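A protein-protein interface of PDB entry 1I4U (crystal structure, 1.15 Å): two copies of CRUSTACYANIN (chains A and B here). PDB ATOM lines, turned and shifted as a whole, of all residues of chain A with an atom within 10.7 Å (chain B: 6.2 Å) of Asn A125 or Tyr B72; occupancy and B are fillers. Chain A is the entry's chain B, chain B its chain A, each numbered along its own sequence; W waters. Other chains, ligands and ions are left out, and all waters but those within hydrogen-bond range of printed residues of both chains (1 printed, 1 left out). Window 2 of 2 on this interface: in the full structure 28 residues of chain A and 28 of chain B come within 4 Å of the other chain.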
ATOM      1  N   VAL A   7      -4.571 -25.948   0.779  1.00  0.00           N
ATOM      2  CA  VAL A   7      -4.730 -25.519   2.204  1.00  0.00           C
ATOM      3  C   VAL A   7      -5.648 -24.296   2.140  1.00  0.00           C
ATOM      4  O   VAL A   7      -5.239 -23.225   1.650  1.00  0.00           O
ATOM      5  CB  VAL A   7      -3.377 -25.210   2.816  1.00  0.00           C
ATOM      6  CG1 VAL A   7      -3.543 -24.638   4.217  1.00  0.00           C
ATOM      7  CG2 VAL A   7      -2.474 -26.449   2.854  1.00  0.00           C
ATOM      8  N   VAL A   8      -6.882 -24.420   2.565  1.00  0.00           N
ATOM      9  CA  VAL A   8      -8.039 -23.535   2.291  1.00  0.00           C
ATOM     10  C   VAL A   8      -8.603 -23.036   3.585  1.00  0.00           C
ATOM     11  O   VAL A   8      -8.659 -23.778   4.561  1.00  0.00           O
ATOM     12  CB  VAL A   8      -9.132 -24.362   1.527  1.00  0.00           C
ATOM     13  CG1 VAL A   8     -10.376 -23.586   1.227  1.00  0.00           C
ATOM     14  CG2 VAL A   8      -8.502 -24.965   0.259  1.00  0.00           C
ATOM     15  N   GLY A  10     -11.027 -22.039   6.701  1.00  0.00           N
ATOM     16  CA  GLY A  10     -12.243 -22.529   7.261  1.00  0.00           C
ATOM     17  C   GLY A  10     -12.208 -24.014   7.544  1.00  0.00           C
ATOM     18  O   GLY A  10     -11.292 -24.764   7.229  1.00  0.00           O
ATOM     19  N   LYS A  11     -13.302 -24.445   8.166  1.00  0.00           N
ATOM     20  CA  LYS A  11     -13.514 -25.841   8.522  1.00  0.00           C
ATOM     21  C   LYS A  11     -13.884 -26.664   7.305  1.00  0.00           C
ATOM     22  O   LYS A  11     -14.515 -26.181   6.336  1.00  0.00           O
ATOM     23  CB  LYS A  11     -14.681 -25.883   9.551  1.00  0.00           C
ATOM     24  CG  LYS A  11     -15.107 -27.204  10.094  1.00  0.00           C
ATOM     25  CD  LYS A  11     -14.273 -27.660  11.234  1.00  0.00           C
ATOM     26  CE  LYS A  11     -14.677 -28.939  11.933  1.00  0.00           C
ATOM     27  NZ  LYS A  11     -14.667 -30.099  10.950  1.00  0.00           N
ATOM     28  N   CYS A  12     -13.579 -27.956   7.345  1.00  0.00           N
ATOM     29  CA  CYS A  12     -14.125 -28.876   6.368  1.00  0.00           C
ATOM     30  C   CYS A  12     -15.648 -28.754   6.257  1.00  0.00           C
ATOM     31  O   CYS A  12     -16.364 -28.616   7.237  1.00  0.00           O
ATOM     32  CB  CYS A  12     -13.801 -30.314   6.784  1.00  0.00           C
ATOM     33  SG  CYS A  12     -12.070 -30.827   6.562  1.00  0.00           S
ATOM     34  N   ILE A 122      -9.458 -32.841   5.698  1.00  0.00           N
ATOM     35  CA  ILE A 122      -8.818 -32.836   6.995  1.00  0.00           C
ATOM     36  C   ILE A 122      -8.739 -31.415   7.525  1.00  0.00           C
ATOM     37  O   ILE A 122      -8.421 -30.494   6.790  1.00  0.00           O
ATOM     38  CB  ILE A 122      -7.427 -33.456   6.976  1.00  0.00           C
ATOM     39  CG1 ILE A 122      -6.747 -33.423   8.341  1.00  0.00           C
ATOM     40  CG2 ILE A 122      -6.519 -32.807   5.975  1.00  0.00           C
ATOM     41  CD1 ILE A 122      -7.363 -34.350   9.380  1.00  0.00           C
ATOM     42  N   ASP A 123      -9.063 -31.259   8.798  1.00  0.00           N
ATOM     43  CA  ASP A 123      -8.981 -30.006   9.512  1.00  0.00           C
ATOM     44  C   ASP A 123      -7.634 -29.804  10.187  1.00  0.00           C
ATOM     45  O   ASP A 123      -7.050 -30.730  10.720  1.00  0.00           O
ATOM     46  CB  ASP A 123     -10.091 -29.948  10.538  1.00  0.00           C
ATOM     47  CG  ASP A 123     -11.454 -29.757   9.919  1.00  0.00           C
ATOM     48  OD1 ASP A 123     -11.629 -28.712   9.268  1.00  0.00           O
ATOM     49  OD2 ASP A 123     -12.293 -30.687  10.064  1.00  0.00           O
ATOM     50  N   TYR A 124      -7.163 -28.563  10.158  1.00  0.00           N
ATOM     51  CA  TYR A 124      -5.951 -28.170  10.871  1.00  0.00           C
ATOM     52  C   TYR A 124      -6.306 -27.382  12.115  1.00  0.00           C
ATOM     53  O   TYR A 124      -7.364 -26.762  12.225  1.00  0.00           O
ATOM     54  CB  TYR A 124      -5.049 -27.309   9.978  1.00  0.00           C
ATOM     55  CG  TYR A 124      -4.609 -28.021   8.696  1.00  0.00           C
ATOM     56  CD1 TYR A 124      -3.811 -29.151   8.739  1.00  0.00           C
ATOM     57  CD2 TYR A 124      -4.977 -27.520   7.472  1.00  0.00           C
ATOM     58  CE1 TYR A 124      -3.404 -29.805   7.584  1.00  0.00           C
ATOM     59  CE2 TYR A 124      -4.582 -28.143   6.289  1.00  0.00           C
ATOM     60  CZ  TYR A 124      -3.792 -29.265   6.371  1.00  0.00           C
ATOM     61  OH  TYR A 124      -3.378 -29.928   5.237  1.00  0.00           O
ATOM     62  N   ASN A 125      -5.366 -27.346  13.048  1.00  0.00           N
ATOM     63  CA  ASN A 125      -5.556 -26.648  14.305  1.00  0.00           C
ATOM     64  C   ASN A 125      -5.467 -25.131  14.192  1.00  0.00           C
ATOM     65  O   ASN A 125      -5.805 -24.454  15.148  1.00  0.00           O
ATOM     66  CB  ASN A 125      -4.613 -27.201  15.362  1.00  0.00           C
ATOM     67  CG  ASN A 125      -3.148 -27.068  15.029  1.00  0.00           C
ATOM     68  OD1 ASN A 125      -2.787 -26.288  14.125  1.00  0.00           O
ATOM     69  ND2 ASN A 125      -2.334 -27.823  15.715  1.00  0.00           N
ATOM     70  N   PHE A 126      -5.130 -24.582  13.050  1.00  0.00           N
ATOM     71  CA  PHE A 126      -5.042 -23.177  12.818  1.00  0.00           C
ATOM     72  C   PHE A 126      -6.258 -22.711  12.022  1.00  0.00           C
ATOM     73  O   PHE A 126      -6.251 -21.560  11.564  1.00  0.00           O
ATOM     74  CB  PHE A 126      -3.709 -22.769  12.206  1.00  0.00           C
ATOM     75  CG  PHE A 126      -3.295 -23.473  10.927  1.00  0.00           C
ATOM     76  CD1 PHE A 126      -2.558 -24.627  10.930  1.00  0.00           C
ATOM     77  CD2 PHE A 126      -3.657 -22.972   9.664  1.00  0.00           C
ATOM     78  CE1 PHE A 126      -2.223 -25.280   9.751  1.00  0.00           C
ATOM     79  CE2 PHE A 126      -3.334 -23.598   8.479  1.00  0.00           C
ATOM     80  CZ  PHE A 126      -2.610 -24.772   8.524  1.00  0.00           C
ATOM     81  N   GLY A 127      -7.278 -23.540  11.886  1.00  0.00           N
ATOM     82  CA  GLY A 127      -8.539 -23.061  11.384  1.00  0.00           C
ATOM     83  C   GLY A 127      -8.758 -23.147   9.883  1.00  0.00           C
ATOM     84  O   GLY A 127      -9.762 -22.662   9.360  1.00  0.00           O
ATOM     85  N   TYR A 128      -7.810 -23.760   9.199  1.00  0.00           N
ATOM     86  CA  TYR A 128      -7.899 -24.072   7.767  1.00  0.00           C
ATOM     87  C   TYR A 128      -8.211 -25.549   7.634  1.00  0.00           C
ATOM     88  O   TYR A 128      -8.254 -26.291   8.609  1.00  0.00           O
ATOM     89  CB  TYR A 128      -6.588 -23.727   7.093  1.00  0.00           C
ATOM     90  CG  TYR A 128      -6.316 -22.302   6.758  1.00  0.00           C
ATOM     91  CD1 TYR A 128      -6.427 -21.279   7.705  1.00  0.00           C
ATOM     92  CD2 TYR A 128      -5.934 -21.954   5.473  1.00  0.00           C
ATOM     93  CE1 TYR A 128      -6.169 -19.984   7.339  1.00  0.00           C
ATOM     94  CE2 TYR A 128      -5.664 -20.646   5.107  1.00  0.00           C
ATOM     95  CZ  TYR A 128      -5.780 -19.670   6.065  1.00  0.00           C
ATOM     96  OH  TYR A 128      -5.529 -18.344   5.714  1.00  0.00           O
ATOM     97  N   HIS A 129      -8.371 -25.981   6.383  1.00  0.00           N
ATOM     98  CA  HIS A 129      -8.540 -27.402   6.069  1.00  0.00           C
ATOM     99  C   HIS A 129      -7.802 -27.662   4.753  1.00  0.00           C
ATOM    100  O   HIS A 129      -7.425 -26.751   4.011  1.00  0.00           O
ATOM    101  CB  HIS A 129     -10.007 -27.786   5.951  1.00  0.00           C
ATOM    102  CG  HIS A 129     -10.744 -27.169   4.785  1.00  0.00           C
ATOM    103  ND1 HIS A 129     -11.257 -25.898   4.856  1.00  0.00           N
ATOM    104  CD2 HIS A 129     -11.084 -27.606   3.555  1.00  0.00           C
ATOM    105  CE1 HIS A 129     -11.864 -25.595   3.717  1.00  0.00           C
ATOM    106  NE2 HIS A 129     -11.774 -26.621   2.881  1.00  0.00           N
ATOM    107  N   SER A 130      -7.622 -28.947   4.485  1.00  0.00           N
ATOM    108  CA  SER A 130      -7.225 -29.396   3.193  1.00  0.00           C
ATOM    109  C   SER A 130      -8.241 -30.422   2.698  1.00  0.00           C
ATOM    110  O   SER A 130      -8.627 -31.316   3.411  1.00  0.00           O
ATOM    111  CB  SER A 130      -5.877 -30.113   3.160  1.00  0.00           C
ATOM    112  OG  SER A 130      -4.870 -29.140   3.218  1.00  0.00           O
ATOM    113  N   ASN B  43       2.883 -29.608  14.761  1.00  0.00           N
ATOM    114  CA  ASN B  43       1.887 -30.593  14.322  1.00  0.00           C
ATOM    115  C   ASN B  43       0.615 -29.828  14.048  1.00  0.00           C
ATOM    116  O   ASN B  43       0.012 -29.299  14.960  1.00  0.00           O
ATOM    117  CB  ASN B  43       1.781 -31.668  15.409  1.00  0.00           C
ATOM    118  CG  ASN B  43       0.841 -32.773  14.985  1.00  0.00           C
ATOM    119  OD1 ASN B  43      -0.176 -32.525  14.327  1.00  0.00           O
ATOM    120  ND2 ASN B  43       1.227 -33.989  15.319  1.00  0.00           N
ATOM    121  N   PRO B  44       0.210 -29.698  12.785  1.00  0.00           N
ATOM    122  CA  PRO B  44      -0.994 -28.910  12.434  1.00  0.00           C
ATOM    123  C   PRO B  44      -2.281 -29.688  12.638  1.00  0.00           C
ATOM    124  O   PRO B  44      -3.352 -29.163  12.403  1.00  0.00           O
ATOM    125  CB  PRO B  44      -0.734 -28.663  10.937  1.00  0.00           C
ATOM    126  CG  PRO B  44      -0.097 -29.946  10.494  1.00  0.00           C
ATOM    127  CD  PRO B  44       0.865 -30.258  11.598  1.00  0.00           C
ATOM    128  N   TYR B  45      -2.184 -30.937  13.096  1.00  0.00           N
ATOM    129  CA  TYR B  45      -3.355 -31.805  13.267  1.00  0.00           C
ATOM    130  C   TYR B  45      -3.783 -31.889  14.718  1.00  0.00           C
ATOM    131  O   TYR B  45      -4.924 -32.221  14.991  1.00  0.00           O
ATOM    132  CB  TYR B  45      -3.038 -33.209  12.768  1.00  0.00           C
ATOM    133  CG  TYR B  45      -2.522 -33.249  11.361  1.00  0.00           C
ATOM    134  CD1 TYR B  45      -3.349 -32.946  10.281  1.00  0.00           C
ATOM    135  CD2 TYR B  45      -1.216 -33.590  11.072  1.00  0.00           C
ATOM    136  CE1 TYR B  45      -2.859 -32.995   8.989  1.00  0.00           C
ATOM    137  CE2 TYR B  45      -0.725 -33.646   9.794  1.00  0.00           C
ATOM    138  CZ  TYR B  45      -1.554 -33.345   8.741  1.00  0.00           C
ATOM    139  OH  TYR B  45      -1.040 -33.394   7.468  1.00  0.00           O
ATOM    140  N   GLN B  46      -2.941 -31.674  15.673  1.00  0.00           N
ATOM    141  CA  GLN B  46      -3.233 -31.809  17.109  1.00  0.00           C
ATOM    142  C   GLN B  46      -4.113 -30.660  17.509  1.00  0.00           C
ATOM    143  O   GLN B  46      -3.703 -29.502  17.542  1.00  0.00           O
ATOM    144  CB  GLN B  46      -1.915 -31.831  17.855  1.00  0.00           C
ATOM    145  CG  GLN B  46      -1.918 -31.642  19.333  1.00  0.00           C
ATOM    146  CD  GLN B  46      -2.590 -32.740  20.099  1.00  0.00           C
ATOM    147  OE1 GLN B  46      -2.016 -33.498  20.887  1.00  0.00           O
ATOM    148  NE2 GLN B  46      -3.869 -32.871  19.862  1.00  0.00           N
ATOM    149  N   LEU B  47      -5.352 -30.971  17.835  1.00  0.00           N
ATOM    150  CA  LEU B  47      -6.327 -29.958  18.240  1.00  0.00           C
ATOM    151  C   LEU B  47      -6.281 -29.552  19.693  1.00  0.00           C
ATOM    152  O   LEU B  47      -6.853 -28.568  20.093  1.00  0.00           O
ATOM    153  CB  LEU B  47      -7.764 -30.448  17.916  1.00  0.00           C
ATOM    154  CG  LEU B  47      -8.045 -30.818  16.461  1.00  0.00           C
ATOM    155  CD1 LEU B  47      -9.494 -31.282  16.317  1.00  0.00           C
ATOM    156  CD2 LEU B  47      -7.671 -29.649  15.557  1.00  0.00           C
ATOM    157  N   ILE B  48      -5.566 -30.266  20.545  1.00  0.00           N
ATOM    158  CA  ILE B  48      -5.385 -29.998  21.920  1.00  0.00           C
ATOM    159  C   ILE B  48      -4.046 -29.313  22.142  1.00  0.00           C
ATOM    160  O   ILE B  48      -2.992 -29.866  21.902  1.00  0.00           O
ATOM    161  CB  ILE B  48      -5.499 -31.275  22.795  1.00  0.00           C
ATOM    162  CG1 ILE B  48      -6.693 -32.150  22.398  1.00  0.00           C
ATOM    163  CG2 ILE B  48      -5.552 -30.923  24.267  1.00  0.00           C
ATOM    164  CD1 ILE B  48      -6.753 -33.472  23.128  1.00  0.00           C
ATOM    165  N   GLU B  49      -4.105 -28.077  22.603  1.00  0.00           N
ATOM    166  CA  GLU B  49      -2.907 -27.259  22.747  1.00  0.00           C
ATOM    167  C   GLU B  49      -2.178 -27.484  24.070  1.00  0.00           C
ATOM    168  O   GLU B  49      -0.942 -27.591  24.106  1.00  0.00           O
ATOM    169  CB  GLU B  49      -3.266 -25.779  22.640  1.00  0.00           C
ATOM    170  CG  GLU B  49      -2.039 -24.895  22.712  1.00  0.00           C
ATOM    171  CD  GLU B  49      -2.276 -23.402  22.604  1.00  0.00           C
ATOM    172  OE1 GLU B  49      -3.431 -22.952  22.864  1.00  0.00           O
ATOM    173  OE2 GLU B  49      -1.323 -22.630  22.335  1.00  0.00           O
ATOM    174  N   ILE B  70      -6.816 -28.557  26.814  1.00  0.00           N
ATOM    175  CA  ILE B  70      -7.367 -27.259  26.442  1.00  0.00           C
ATOM    176  C   ILE B  70      -7.101 -27.049  24.951  1.00  0.00           C
ATOM    177  O   ILE B  70      -5.940 -27.117  24.534  1.00  0.00           O
ATOM    178  CB  ILE B  70      -6.749 -26.103  27.259  1.00  0.00           C
ATOM    179  CG1 ILE B  70      -6.660 -26.401  28.749  1.00  0.00           C
ATOM    180  CG2 ILE B  70      -7.511 -24.819  26.987  1.00  0.00           C
ATOM    181  CD1 ILE B  70      -8.021 -26.704  29.291  1.00  0.00           C
ATOM    182  N   ALA B  71      -8.148 -26.780  24.197  1.00  0.00           N
ATOM    183  CA  ALA B  71      -8.103 -26.551  22.752  1.00  0.00           C
ATOM    184  C   ALA B  71      -7.514 -25.176  22.487  1.00  0.00           C
ATOM    185  O   ALA B  71      -7.352 -24.374  23.432  1.00  0.00           O
ATOM    186  CB  ALA B  71      -9.517 -26.628  22.228  1.00  0.00           C
ATOM    187  N   TYR B  72      -7.209 -24.897  21.220  1.00  0.00           N
ATOM    188  CA  TYR B  72      -6.617 -23.618  20.830  1.00  0.00           C
ATOM    189  C   TYR B  72      -7.528 -22.421  21.080  1.00  0.00           C
ATOM    190  O   TYR B  72      -7.046 -21.289  21.204  1.00  0.00           O
ATOM    191  CB  TYR B  72      -6.143 -23.697  19.365  1.00  0.00           C
ATOM    192  CG  TYR B  72      -4.844 -24.471  19.250  1.00  0.00           C
ATOM    193  CD1 TYR B  72      -4.832 -25.868  19.065  1.00  0.00           C
ATOM    194  CD2 TYR B  72      -3.602 -23.844  19.365  1.00  0.00           C
ATOM    195  CE1 TYR B  72      -3.645 -26.551  18.977  1.00  0.00           C
ATOM    196  CE2 TYR B  72      -2.419 -24.523  19.289  1.00  0.00           C
ATOM    197  CZ  TYR B  72      -2.447 -25.881  19.086  1.00  0.00           C
ATOM    198  OH  TYR B  72      -1.259 -26.576  19.020  1.00  0.00           O
ATOM    199  N   ASP B  73      -8.826 -22.635  21.225  1.00  0.00           N
ATOM    200  CA  ASP B  73      -9.757 -21.567  21.531  1.00  0.00           C
ATOM    201  C   ASP B  73      -9.908 -21.362  23.036  1.00  0.00           C
ATOM    202  O   ASP B  73     -10.687 -20.531  23.507  1.00  0.00           O
ATOM    203  CB  ASP B  73     -11.133 -21.820  20.924  1.00  0.00           C
ATOM    204  CG  ASP B  73     -11.871 -23.047  21.421  1.00  0.00           C
ATOM    205  OD1 ASP B  73     -11.354 -23.798  22.269  1.00  0.00           O
ATOM    206  OD2 ASP B  73     -13.003 -23.230  20.890  1.00  0.00           O
ATOM    207  N   GLY B  74      -9.235 -22.142  23.844  1.00  0.00           N
ATOM    208  CA  GLY B  74      -9.364 -22.034  25.259  1.00  0.00           C
ATOM    209  C   GLY B  74     -10.382 -22.922  25.947  1.00  0.00           C
ATOM    210  O   GLY B  74     -10.468 -22.881  27.198  1.00  0.00           O
ATOM    211  N   ASN B  75     -11.149 -23.706  25.208  1.00  0.00           N
ATOM    212  CA  ASN B  75     -12.137 -24.582  25.837  1.00  0.00           C
ATOM    213  C   ASN B  75     -11.549 -25.942  26.120  1.00  0.00           C
ATOM    214  O   ASN B  75     -10.676 -26.407  25.398  1.00  0.00           O
ATOM    215  CB  ASN B  75     -13.398 -24.724  24.977  1.00  0.00           C
ATOM    216  CG  ASN B  75     -14.046 -23.334  24.950  1.00  0.00           C
ATOM    217  OD1 ASN B  75     -14.261 -22.781  26.011  1.00  0.00           O
ATOM    218  ND2 ASN B  75     -14.278 -22.870  23.743  1.00  0.00           N
HETATM  219  O   HOH W   1      -2.856 -32.888   5.503  1.00  0.00           O
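ND2 of Asn A125 lies within hydrogen-bond range of O of Asn B43, 2.9 Å away.
The backbone carbonyl oxygen (O) of Gln B46 lies within hydrogen-bond range of the side-chain amide nitrogen (ND2) of Asn A125, at 2.8 Å.
O of Pro B44 sits at hydrogen-bond distance from N of Asn A125 (2.8 Å).
Ile A122 touches Tyr B45 (CG1 to CD1, 3.9 Å).
CA of Tyr A124 touches O of Pro B44 (3.2 Å).
CE1 of Tyr B45 touches CE1 of Tyr A124, at 3.5 Å.
Asn A125 touches Leu B47 (CA to CD2, 3.9 Å).
Asn A125 touches Tyr B72.
Phe A126 touches Pro B44.
OH of Tyr A124 is in hydrogen-bond range of OG of Ser A130 (2.6 Å).
NE2 of Gln B46 sits close to N of Ile B48, at 3.2 Å.
N of Ile A122 lies within hydrogen-bond range of O of Ser A130.
The side-chain amide oxygen (OD1) of Asn B43 is in hydrogen-bond range of the backbone NH (N) of Gln B46 (3.2 Å).
The side-chain amide oxygen (OD1) of Asn B43 is in hydrogen-bond range of the backbone NH (N) of Tyr B45 (2.8 Å).
SG of Cys A12 sits at hydrogen-bond distance from N of Ile A122 (3.4 Å).
Of the 14 printed residues of chain A, 4 touch a printed residue of chain B.
Printed residues of chain A that touch a printed residue of chain B: Ile A122, Tyr A124, Asn A125 and Phe A126.
Hydrophobic or aromatic side chains of chain A within 4 Å of the printed part of chain B: Ile A122, Tyr A124 and Phe A126.
Printed residues of chain B that touch a printed residue of chain A: Asn B43, Pro B44, Tyr B45, Gln B46, Leu B47 and Tyr B72.
Hydrophobic or aromatic side chains of chain B that line the printed part of chain A: Pro B44, Tyr B45, Leu B47 and Tyr B72.
Among the printed residues, no Asp or Glu carboxylate lies within 4 Å of a Lys or Arg side-chain nitrogen of the other chain.
Of the printed residues of chain B, Ile A122 touches Tyr B45 (3.9 Å).
Of the printed residues of chain B, Tyr A124 touches Pro B44 (3.2 Å) and Tyr B45 (3.5 Å).
Asn A125 touches just these residues of chain B: Asn B43, Pro B44, Gln B46, Leu B47 and Tyr B72.
Of the printed residues of chain A, Asn B43 touches Asn A125.
Pro B44 touches three residues of chain A.
Of the printed residues of chain A, Tyr B45 touches Ile A122 and Tyr A124.
Printed residues of chain A within 4 Å of Gln B46: Asn A125 (2.8 Å).
Of chain A, only Asn A125 comes within 4 Å of Leu B47.
No residue of chain A comes within 4 Å of Glu B49.
No residue of chain A comes within 4 Å of Ala B71.
Tyr B72 touches one residue of chain A.
No residue of chain A comes within 4 Å of Asp B73.
The nearest residue of chain A that does not touch Tyr B72 is Phe A126 (6.2 Å).
Water W1 bridges OH of Tyr B45 (2.7 Å) and OH of Tyr A124 (3.0 Å).
No position is printed for both chains.
Of the 9 pairs that touch across the chains among the printed residues, none has its exchanged pair printed and touching as well.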
